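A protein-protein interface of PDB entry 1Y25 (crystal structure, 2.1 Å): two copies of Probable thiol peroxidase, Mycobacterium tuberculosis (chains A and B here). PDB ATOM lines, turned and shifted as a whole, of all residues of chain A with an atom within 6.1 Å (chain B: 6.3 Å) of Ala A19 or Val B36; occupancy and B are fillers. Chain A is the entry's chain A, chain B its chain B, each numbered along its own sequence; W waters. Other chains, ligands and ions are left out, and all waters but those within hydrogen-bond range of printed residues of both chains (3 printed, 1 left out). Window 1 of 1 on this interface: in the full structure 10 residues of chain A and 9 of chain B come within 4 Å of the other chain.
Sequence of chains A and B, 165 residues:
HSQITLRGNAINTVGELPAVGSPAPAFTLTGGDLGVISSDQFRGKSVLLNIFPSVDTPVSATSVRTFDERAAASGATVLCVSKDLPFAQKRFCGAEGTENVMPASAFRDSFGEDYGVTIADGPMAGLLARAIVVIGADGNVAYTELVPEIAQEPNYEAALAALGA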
ATOM      1  N   GLY A  15       2.150   5.970 -26.368  1.00  0.00           N
ATOM      2  CA  GLY A  15       3.332   5.165 -26.656  1.00  0.00           C
ATOM      3  C   GLY A  15       3.105   3.747 -26.279  1.00  0.00           C
ATOM      4  O   GLY A  15       2.002   3.255 -26.419  1.00  0.00           O
ATOM      5  N   GLU A  16       4.158   3.100 -25.777  1.00  0.00           N
ATOM      6  CA  GLU A  16       4.148   1.666 -25.478  1.00  0.00           C
ATOM      7  C   GLU A  16       4.775   1.355 -24.087  1.00  0.00           C
ATOM      8  O   GLU A  16       5.709   2.035 -23.635  1.00  0.00           O
ATOM      9  CB  GLU A  16       4.853   0.871 -26.582  1.00  0.00           C
ATOM     10  CG  GLU A  16       3.966   0.381 -27.781  1.00  0.00           C
ATOM     11  CD  GLU A  16       4.812  -0.334 -28.923  1.00  0.00           C
ATOM     12  OE1 GLU A  16       4.413  -1.474 -29.391  1.00  0.00           O
ATOM     13  OE2 GLU A  16       5.841   0.265 -29.376  1.00  0.00           O
ATOM     14  N   LEU A  17       4.261   0.280 -23.499  1.00  0.00           N
ATOM     15  CA  LEU A  17       4.728  -0.254 -22.239  1.00  0.00           C
ATOM     16  C   LEU A  17       6.117  -0.888 -22.522  1.00  0.00           C
ATOM     17  O   LEU A  17       6.417  -1.317 -23.651  1.00  0.00           O
ATOM     18  CB  LEU A  17       3.739  -1.318 -21.722  1.00  0.00           C
ATOM     19  CG  LEU A  17       2.405  -0.794 -21.131  1.00  0.00           C
ATOM     20  CD1 LEU A  17       1.487  -1.945 -20.761  1.00  0.00           C
ATOM     21  CD2 LEU A  17       2.754   0.043 -19.910  1.00  0.00           C
ATOM     22  N   PRO A  18       6.974  -0.901 -21.507  1.00  0.00           N
ATOM     23  CA  PRO A  18       8.363  -1.429 -21.725  1.00  0.00           C
ATOM     24  C   PRO A  18       8.306  -2.927 -21.840  1.00  0.00           C
ATOM     25  O   PRO A  18       7.445  -3.504 -21.229  1.00  0.00           O
ATOM     26  CB  PRO A  18       9.110  -0.951 -20.459  1.00  0.00           C
ATOM     27  CG  PRO A  18       8.052  -0.817 -19.459  1.00  0.00           C
ATOM     28  CD  PRO A  18       6.795  -0.367 -20.155  1.00  0.00           C
ATOM     29  N   ALA A  19       9.138  -3.521 -22.691  1.00  0.00           N
ATOM     30  CA  ALA A  19       9.325  -4.989 -22.736  1.00  0.00           C
ATOM     31  C   ALA A  19       9.740  -5.640 -21.407  1.00  0.00           C
ATOM     32  O   ALA A  19      10.685  -5.204 -20.686  1.00  0.00           O
ATOM     33  CB  ALA A  19      10.317  -5.310 -23.733  1.00  0.00           C
ATOM     34  N   VAL A  20       9.071  -6.725 -21.105  1.00  0.00           N
ATOM     35  CA  VAL A  20       9.496  -7.652 -20.032  1.00  0.00           C
ATOM     36  C   VAL A  20      10.992  -7.957 -20.241  1.00  0.00           C
ATOM     37  O   VAL A  20      11.402  -8.143 -21.372  1.00  0.00           O
ATOM     38  CB  VAL A  20       8.561  -8.849 -20.046  1.00  0.00           C
ATOM     39  CG1 VAL A  20       9.141 -10.010 -19.287  1.00  0.00           C
ATOM     40  CG2 VAL A  20       7.214  -8.475 -19.488  1.00  0.00           C
ATOM     41  N   GLY A  21      11.788  -7.801 -19.179  1.00  0.00           N
ATOM     42  CA  GLY A  21      13.189  -8.066 -19.153  1.00  0.00           C
ATOM     43  C   GLY A  21      14.050  -6.810 -19.262  1.00  0.00           C
ATOM     44  O   GLY A  21      15.209  -6.826 -18.919  1.00  0.00           O
ATOM     45  N   SER A  22      13.480  -5.733 -19.758  1.00  0.00           N
ATOM     46  CA  SER A  22      14.134  -4.472 -19.883  1.00  0.00           C
ATOM     47  C   SER A  22      13.979  -3.641 -18.571  1.00  0.00           C
ATOM     48  O   SER A  22      13.152  -3.960 -17.750  1.00  0.00           O
ATOM     49  CB  SER A  22      13.596  -3.719 -21.127  1.00  0.00           C
ATOM     50  OG  SER A  22      12.310  -3.166 -20.899  1.00  0.00           O
ATOM     51  N   PRO A  23      14.888  -2.633 -18.342  1.00  0.00           N
ATOM     52  CA  PRO A  23      14.851  -1.789 -17.127  1.00  0.00           C
ATOM     53  C   PRO A  23      13.563  -0.997 -17.080  1.00  0.00           C
ATOM     54  O   PRO A  23      13.194  -0.275 -18.042  1.00  0.00           O
ATOM     55  CB  PRO A  23      16.059  -0.885 -17.266  1.00  0.00           C
ATOM     56  CG  PRO A  23      16.968  -1.578 -18.375  1.00  0.00           C
ATOM     57  CD  PRO A  23      15.981  -2.251 -19.255  1.00  0.00           C
ATOM     58  N   VAL A 141      11.563  -5.090 -15.851  1.00  0.00           N
ATOM     59  CA  VAL A 141      10.110  -5.283 -15.968  1.00  0.00           C
ATOM     60  C   VAL A 141       9.919  -6.816 -15.946  1.00  0.00           C
ATOM     61  O   VAL A 141      10.529  -7.525 -16.781  1.00  0.00           O
ATOM     62  CB  VAL A 141       9.606  -4.720 -17.292  1.00  0.00           C
ATOM     63  CG1 VAL A 141       8.170  -5.010 -17.498  1.00  0.00           C
ATOM     64  CG2 VAL A 141       9.822  -3.235 -17.401  1.00  0.00           C
ATOM     65  N   THR A 144       3.682  -7.207 -17.709  1.00  0.00           N
ATOM     66  CA  THR A 144       2.886  -6.168 -18.166  1.00  0.00           C
ATOM     67  C   THR A 144       1.549  -6.721 -18.663  1.00  0.00           C
ATOM     68  O   THR A 144       1.465  -7.885 -19.152  1.00  0.00           O
ATOM     69  CB  THR A 144       3.567  -5.302 -19.324  1.00  0.00           C
ATOM     70  OG1 THR A 144       3.783  -6.070 -20.550  1.00  0.00           O
ATOM     71  CG2 THR A 144       4.847  -4.688 -18.775  1.00  0.00           C
ATOM     72  N   PHE B  27      17.534   5.677 -29.046  1.00  0.00           N
ATOM     73  CA  PHE B  27      16.926   4.576 -29.771  1.00  0.00           C
ATOM     74  C   PHE B  27      15.623   4.093 -29.131  1.00  0.00           C
ATOM     75  O   PHE B  27      15.425   4.238 -27.914  1.00  0.00           O
ATOM     76  CB  PHE B  27      17.924   3.431 -29.988  1.00  0.00           C
ATOM     77  CG  PHE B  27      18.492   2.828 -28.726  1.00  0.00           C
ATOM     78  CD1 PHE B  27      17.707   2.074 -27.866  1.00  0.00           C
ATOM     79  CD2 PHE B  27      19.829   2.918 -28.460  1.00  0.00           C
ATOM     80  CE1 PHE B  27      18.230   1.458 -26.819  1.00  0.00           C
ATOM     81  CE2 PHE B  27      20.349   2.354 -27.340  1.00  0.00           C
ATOM     82  CZ  PHE B  27      19.573   1.614 -26.540  1.00  0.00           C
ATOM     83  N   THR B  28      14.720   3.588 -29.962  1.00  0.00           N
ATOM     84  CA  THR B  28      13.554   2.874 -29.481  1.00  0.00           C
ATOM     85  C   THR B  28      13.517   1.531 -30.237  1.00  0.00           C
ATOM     86  O   THR B  28      13.350   1.491 -31.419  1.00  0.00           O
ATOM     87  CB  THR B  28      12.194   3.668 -29.703  1.00  0.00           C
ATOM     88  OG1 THR B  28      11.825   3.558 -31.071  1.00  0.00           O
ATOM     89  CG2 THR B  28      12.282   5.093 -29.361  1.00  0.00           C
ATOM     90  N   LEU B  29      13.749   0.424 -29.552  1.00  0.00           N
ATOM     91  CA  LEU B  29      13.851  -0.879 -30.180  1.00  0.00           C
ATOM     92  C   LEU B  29      12.663  -1.677 -29.716  1.00  0.00           C
ATOM     93  O   LEU B  29      11.887  -1.212 -28.891  1.00  0.00           O
ATOM     94  CB  LEU B  29      15.192  -1.528 -29.772  1.00  0.00           C
ATOM     95  CG  LEU B  29      16.504  -0.994 -30.393  1.00  0.00           C
ATOM     96  CD1 LEU B  29      17.692  -1.333 -29.597  1.00  0.00           C
ATOM     97  CD2 LEU B  29      16.698  -1.417 -31.797  1.00  0.00           C
ATOM     98  N   THR B  30      12.506  -2.859 -30.266  1.00  0.00           N
ATOM     99  CA  THR B  30      11.426  -3.752 -29.911  1.00  0.00           C
ATOM    100  C   THR B  30      11.907  -4.959 -29.118  1.00  0.00           C
ATOM    101  O   THR B  30      12.745  -5.723 -29.583  1.00  0.00           O
ATOM    102  CB  THR B  30      10.643  -4.244 -31.164  1.00  0.00           C
ATOM    103  OG1 THR B  30      10.188  -3.103 -31.916  1.00  0.00           O
ATOM    104  CG2 THR B  30       9.445  -5.066 -30.744  1.00  0.00           C
ATOM    105  N   GLY B  31      11.306  -5.118 -27.936  1.00  0.00           N
ATOM    106  CA  GLY B  31      11.538  -6.232 -27.042  1.00  0.00           C
ATOM    107  C   GLY B  31      10.896  -7.520 -27.445  1.00  0.00           C
ATOM    108  O   GLY B  31      10.078  -7.561 -28.395  1.00  0.00           O
ATOM    109  N   GLY B  32      11.297  -8.586 -26.738  1.00  0.00           N
ATOM    110  CA  GLY B  32      10.887  -9.951 -27.096  1.00  0.00           C
ATOM    111  C   GLY B  32       9.426 -10.203 -27.113  1.00  0.00           C
ATOM    112  O   GLY B  32       8.965 -11.023 -27.888  1.00  0.00           O
ATOM    113  N   ASP B  33       8.719  -9.480 -26.255  1.00  0.00           N
ATOM    114  CA  ASP B  33       7.266  -9.523 -26.061  1.00  0.00           C
ATOM    115  C   ASP B  33       6.525  -8.461 -26.868  1.00  0.00           C
ATOM    116  O   ASP B  33       5.375  -8.302 -26.678  1.00  0.00           O
ATOM    117  CB  ASP B  33       6.912  -9.398 -24.563  1.00  0.00           C
ATOM    118  CG  ASP B  33       7.287  -7.983 -23.929  1.00  0.00           C
ATOM    119  OD1 ASP B  33       7.890  -7.114 -24.537  1.00  0.00           O
ATOM    120  OD2 ASP B  33       6.887  -7.767 -22.827  1.00  0.00           O
ATOM    121  N   LEU B  34       7.243  -7.760 -27.753  1.00  0.00           N
ATOM    122  CA  LEU B  34       6.793  -6.681 -28.648  1.00  0.00           C
ATOM    123  C   LEU B  34       6.612  -5.353 -27.939  1.00  0.00           C
ATOM    124  O   LEU B  34       6.213  -4.375 -28.561  1.00  0.00           O
ATOM    125  CB  LEU B  34       5.543  -7.047 -29.458  1.00  0.00           C
ATOM    126  CG  LEU B  34       5.659  -8.388 -30.211  1.00  0.00           C
ATOM    127  CD1 LEU B  34       4.406  -8.709 -30.924  1.00  0.00           C
ATOM    128  CD2 LEU B  34       6.855  -8.390 -31.197  1.00  0.00           C
ATOM    129  N   GLY B  35       6.937  -5.323 -26.658  1.00  0.00           N
ATOM    130  CA  GLY B  35       7.172  -4.035 -25.943  1.00  0.00           C
ATOM    131  C   GLY B  35       8.334  -3.203 -26.420  1.00  0.00           C
ATOM    132  O   GLY B  35       9.285  -3.651 -27.068  1.00  0.00           O
ATOM    133  N   VAL B  36       8.322  -1.961 -26.047  1.00  0.00           N
ATOM    134  CA  VAL B  36       9.484  -1.128 -26.385  1.00  0.00           C
ATOM    135  C   VAL B  36      10.653  -1.252 -25.428  1.00  0.00           C
ATOM    136  O   VAL B  36      10.493  -1.586 -24.262  1.00  0.00           O
ATOM    137  CB  VAL B  36       9.043   0.343 -26.573  1.00  0.00           C
ATOM    138  CG1 VAL B  36      10.132   1.233 -27.044  1.00  0.00           C
ATOM    139  CG2 VAL B  36       7.976   0.376 -27.597  1.00  0.00           C
ATOM    140  N   ILE B  37      11.829  -1.034 -25.983  1.00  0.00           N
ATOM    141  CA  ILE B  37      13.101  -0.885 -25.280  1.00  0.00           C
ATOM    142  C   ILE B  37      13.723   0.420 -25.792  1.00  0.00           C
ATOM    143  O   ILE B  37      14.233   0.499 -26.908  1.00  0.00           O
ATOM    144  CB  ILE B  37      14.064  -2.043 -25.445  1.00  0.00           C
ATOM    145  CG1 ILE B  37      13.391  -3.351 -24.968  1.00  0.00           C
ATOM    146  CG2 ILE B  37      15.242  -1.861 -24.629  1.00  0.00           C
ATOM    147  CD1 ILE B  37      14.297  -4.567 -24.952  1.00  0.00           C
ATOM    148  N   SER B  38      13.621   1.429 -24.947  1.00  0.00           N
ATOM    149  CA  SER B  38      14.046   2.765 -25.204  1.00  0.00           C
ATOM    150  C   SER B  38      15.394   2.984 -24.503  1.00  0.00           C
ATOM    151  O   SER B  38      15.616   2.472 -23.380  1.00  0.00           O
ATOM    152  CB  SER B  38      13.063   3.755 -24.622  1.00  0.00           C
ATOM    153  OG  SER B  38      13.568   5.085 -24.831  1.00  0.00           O
ATOM    154  N   GLN B  41      15.385   4.131 -20.944  1.00  0.00           N
ATOM    155  CA  GLN B  41      15.439   3.173 -19.871  1.00  0.00           C
ATOM    156  C   GLN B  41      16.887   2.940 -19.296  1.00  0.00           C
ATOM    157  O   GLN B  41      17.030   2.456 -18.184  1.00  0.00           O
ATOM    158  CB  GLN B  41      14.796   1.861 -20.302  1.00  0.00           C
ATOM    159  CG  GLN B  41      13.262   1.931 -20.469  1.00  0.00           C
ATOM    160  CD  GLN B  41      12.670   0.786 -21.298  1.00  0.00           C
ATOM    161  OE1 GLN B  41      12.614  -0.337 -20.847  1.00  0.00           O
ATOM    162  NE2 GLN B  41      12.174   1.089 -22.462  1.00  0.00           N
ATOM    163  N   ARG B 108      11.637  -2.672 -37.001  1.00  0.00           N
ATOM    164  CA  ARG B 108      10.696  -1.537 -37.298  1.00  0.00           C
ATOM    165  C   ARG B 108      11.272  -0.205 -36.754  1.00  0.00           C
ATOM    166  O   ARG B 108      10.531   0.688 -36.393  1.00  0.00           O
ATOM    167  CB  ARG B 108       9.267  -1.772 -36.716  1.00  0.00           C
ATOM    168  CG  ARG B 108       9.355  -2.201 -35.308  1.00  0.00           C
ATOM    169  CD  ARG B 108       8.195  -1.988 -34.386  1.00  0.00           C
ATOM    170  NE  ARG B 108       7.096  -2.903 -34.520  1.00  0.00           N
ATOM    171  CZ  ARG B 108       6.384  -3.461 -33.538  1.00  0.00           C
ATOM    172  NH1 ARG B 108       6.628  -3.327 -32.252  1.00  0.00           N
ATOM    173  NH2 ARG B 108       5.383  -4.228 -33.881  1.00  0.00           N
HETATM  174  O   HOH W   1      10.318  -9.539 -23.449  1.00  0.00           O
HETATM  175  O   HOH W   2       7.429  -2.092 -29.766  1.00  0.00           O
HETATM  176  O   HOH W   3       5.581  -5.588 -22.216  1.00  0.00           O
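The backbone carbonyl oxygen (O) of Val B36 is in hydrogen-bond range of the backbone NH (N) of Ala A19, at 2.8 Å. The backbone carbonyl oxygen (O) of Leu A17 lies within hydrogen-bond range of the backbone NH (N) of Val B36 (3.1 Å). The side-chain hydroxyl (OG) of Ser A22 lies within hydrogen-bond range of the side-chain amide oxygen (OE1) of Gln B41 (2.8 Å). The backbone carbonyl oxygen (O) of Pro A23 lies close to the side-chain amide oxygen (OE1) of Gln B41 (2.9 Å). N of Val A20 is in hydrogen-bond range of OD2 of Asp B33.
O of Ala A19 lies within hydrogen-bond range of OG of Ser A22 (2.6 Å). OD1 of Asp B33 sits at hydrogen-bond distance from N of Gly B35 (2.9 Å). The backbone carbonyl oxygen of Ser A22 sits at hydrogen-bond distance from the backbone NH of Val A141. The side-chain amide nitrogen (NE2) of Gln B41 sits close to the backbone NH (N) of Ser B38. The backbone NH of Leu B29 is in hydrogen-bond range of the backbone carbonyl oxygen of Ile B37.
Glu A16 touches Leu B34 (OE1 to O, 3.5 Å). Glu A16 touches Val B36 (OE2 to CG2, 2.8 Å). Leu A17 touches Gly B35 (O to CA, 3.6 Å). Pro A18 touches Val B36 (CA to O, 3.3 Å). Gln B41 touches Pro A18. Ala A19 touches Gly B31. Asp B33 touches Ala A19 (OD1 to CB, 3.1 Å). Ala A19 touches Gly B35 (N to C, 3.8 Å). Ala A19 touches Ile B37. Ser A22 touches Ile B37.
Printed residues of chain B within 4 Å of Leu A17: Gly B35 (3.6 Å) and Val B36 (3.1 Å). Of the printed residues of chain B, Pro A18 touches Val B36 (3.3 Å) and Gln B41 (3.6 Å). Ala A19 touches five residues of chain B. Of the printed residues of chain A, Gly B35 touches Leu A17 and Ala A19. Val B36 touches just these residues of chain A: Glu A16, Leu A17, Pro A18 and Ala A19. Of the printed residues of chain A, Ile B37 touches Ala A19 (3.8 Å) and Ser A22 (3.9 Å). Printed residues of chain A within 4 Å of Gln B41: Pro A18, Ser A22 and Pro A23. The nearest residue of chain B that does not touch Ala A19 is Gly B32 (4.6 Å). The nearest printed residue of chain A that does not touch Gln B41 is Ala A19 (5.1 Å).
Printed residues of chain B that touch a printed residue of chain A: Gly B31, Asp B33, Leu B34, Gly B35, Val B36, Ile B37 and Gln B41. Hydrophobic or aromatic side chains of chain A within 4 Å of the printed part of chain B: Pro A18, Ala A19, Val A20 and Pro A23. Among the printed residues, 15 pairs touch across the chains.
No position is printed for both chains. Of the 15 pairs that touch across the chains among the printed residues, none has its exchanged pair printed and touching as well.
Water W3 lies within hydrogen-bond range of the side-chain hydroxyl (OG1) of Thr A144, the side-chain carboxylate (OD2) of Asp B33 and the backbone carbonyl oxygen (O) of Pro A18. Water W1 lies within hydrogen-bond range of the backbone carbonyl oxygen of Val A20 and the backbone NH of Asp B33. Water W2 lies within hydrogen-bond range of the backbone carbonyl oxygen of Leu B34 (2.9 Å), the side-chain carboxylate of Glu A16 (2.9 Å) and the guanidinium group of Arg B108 (2.9 Å).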
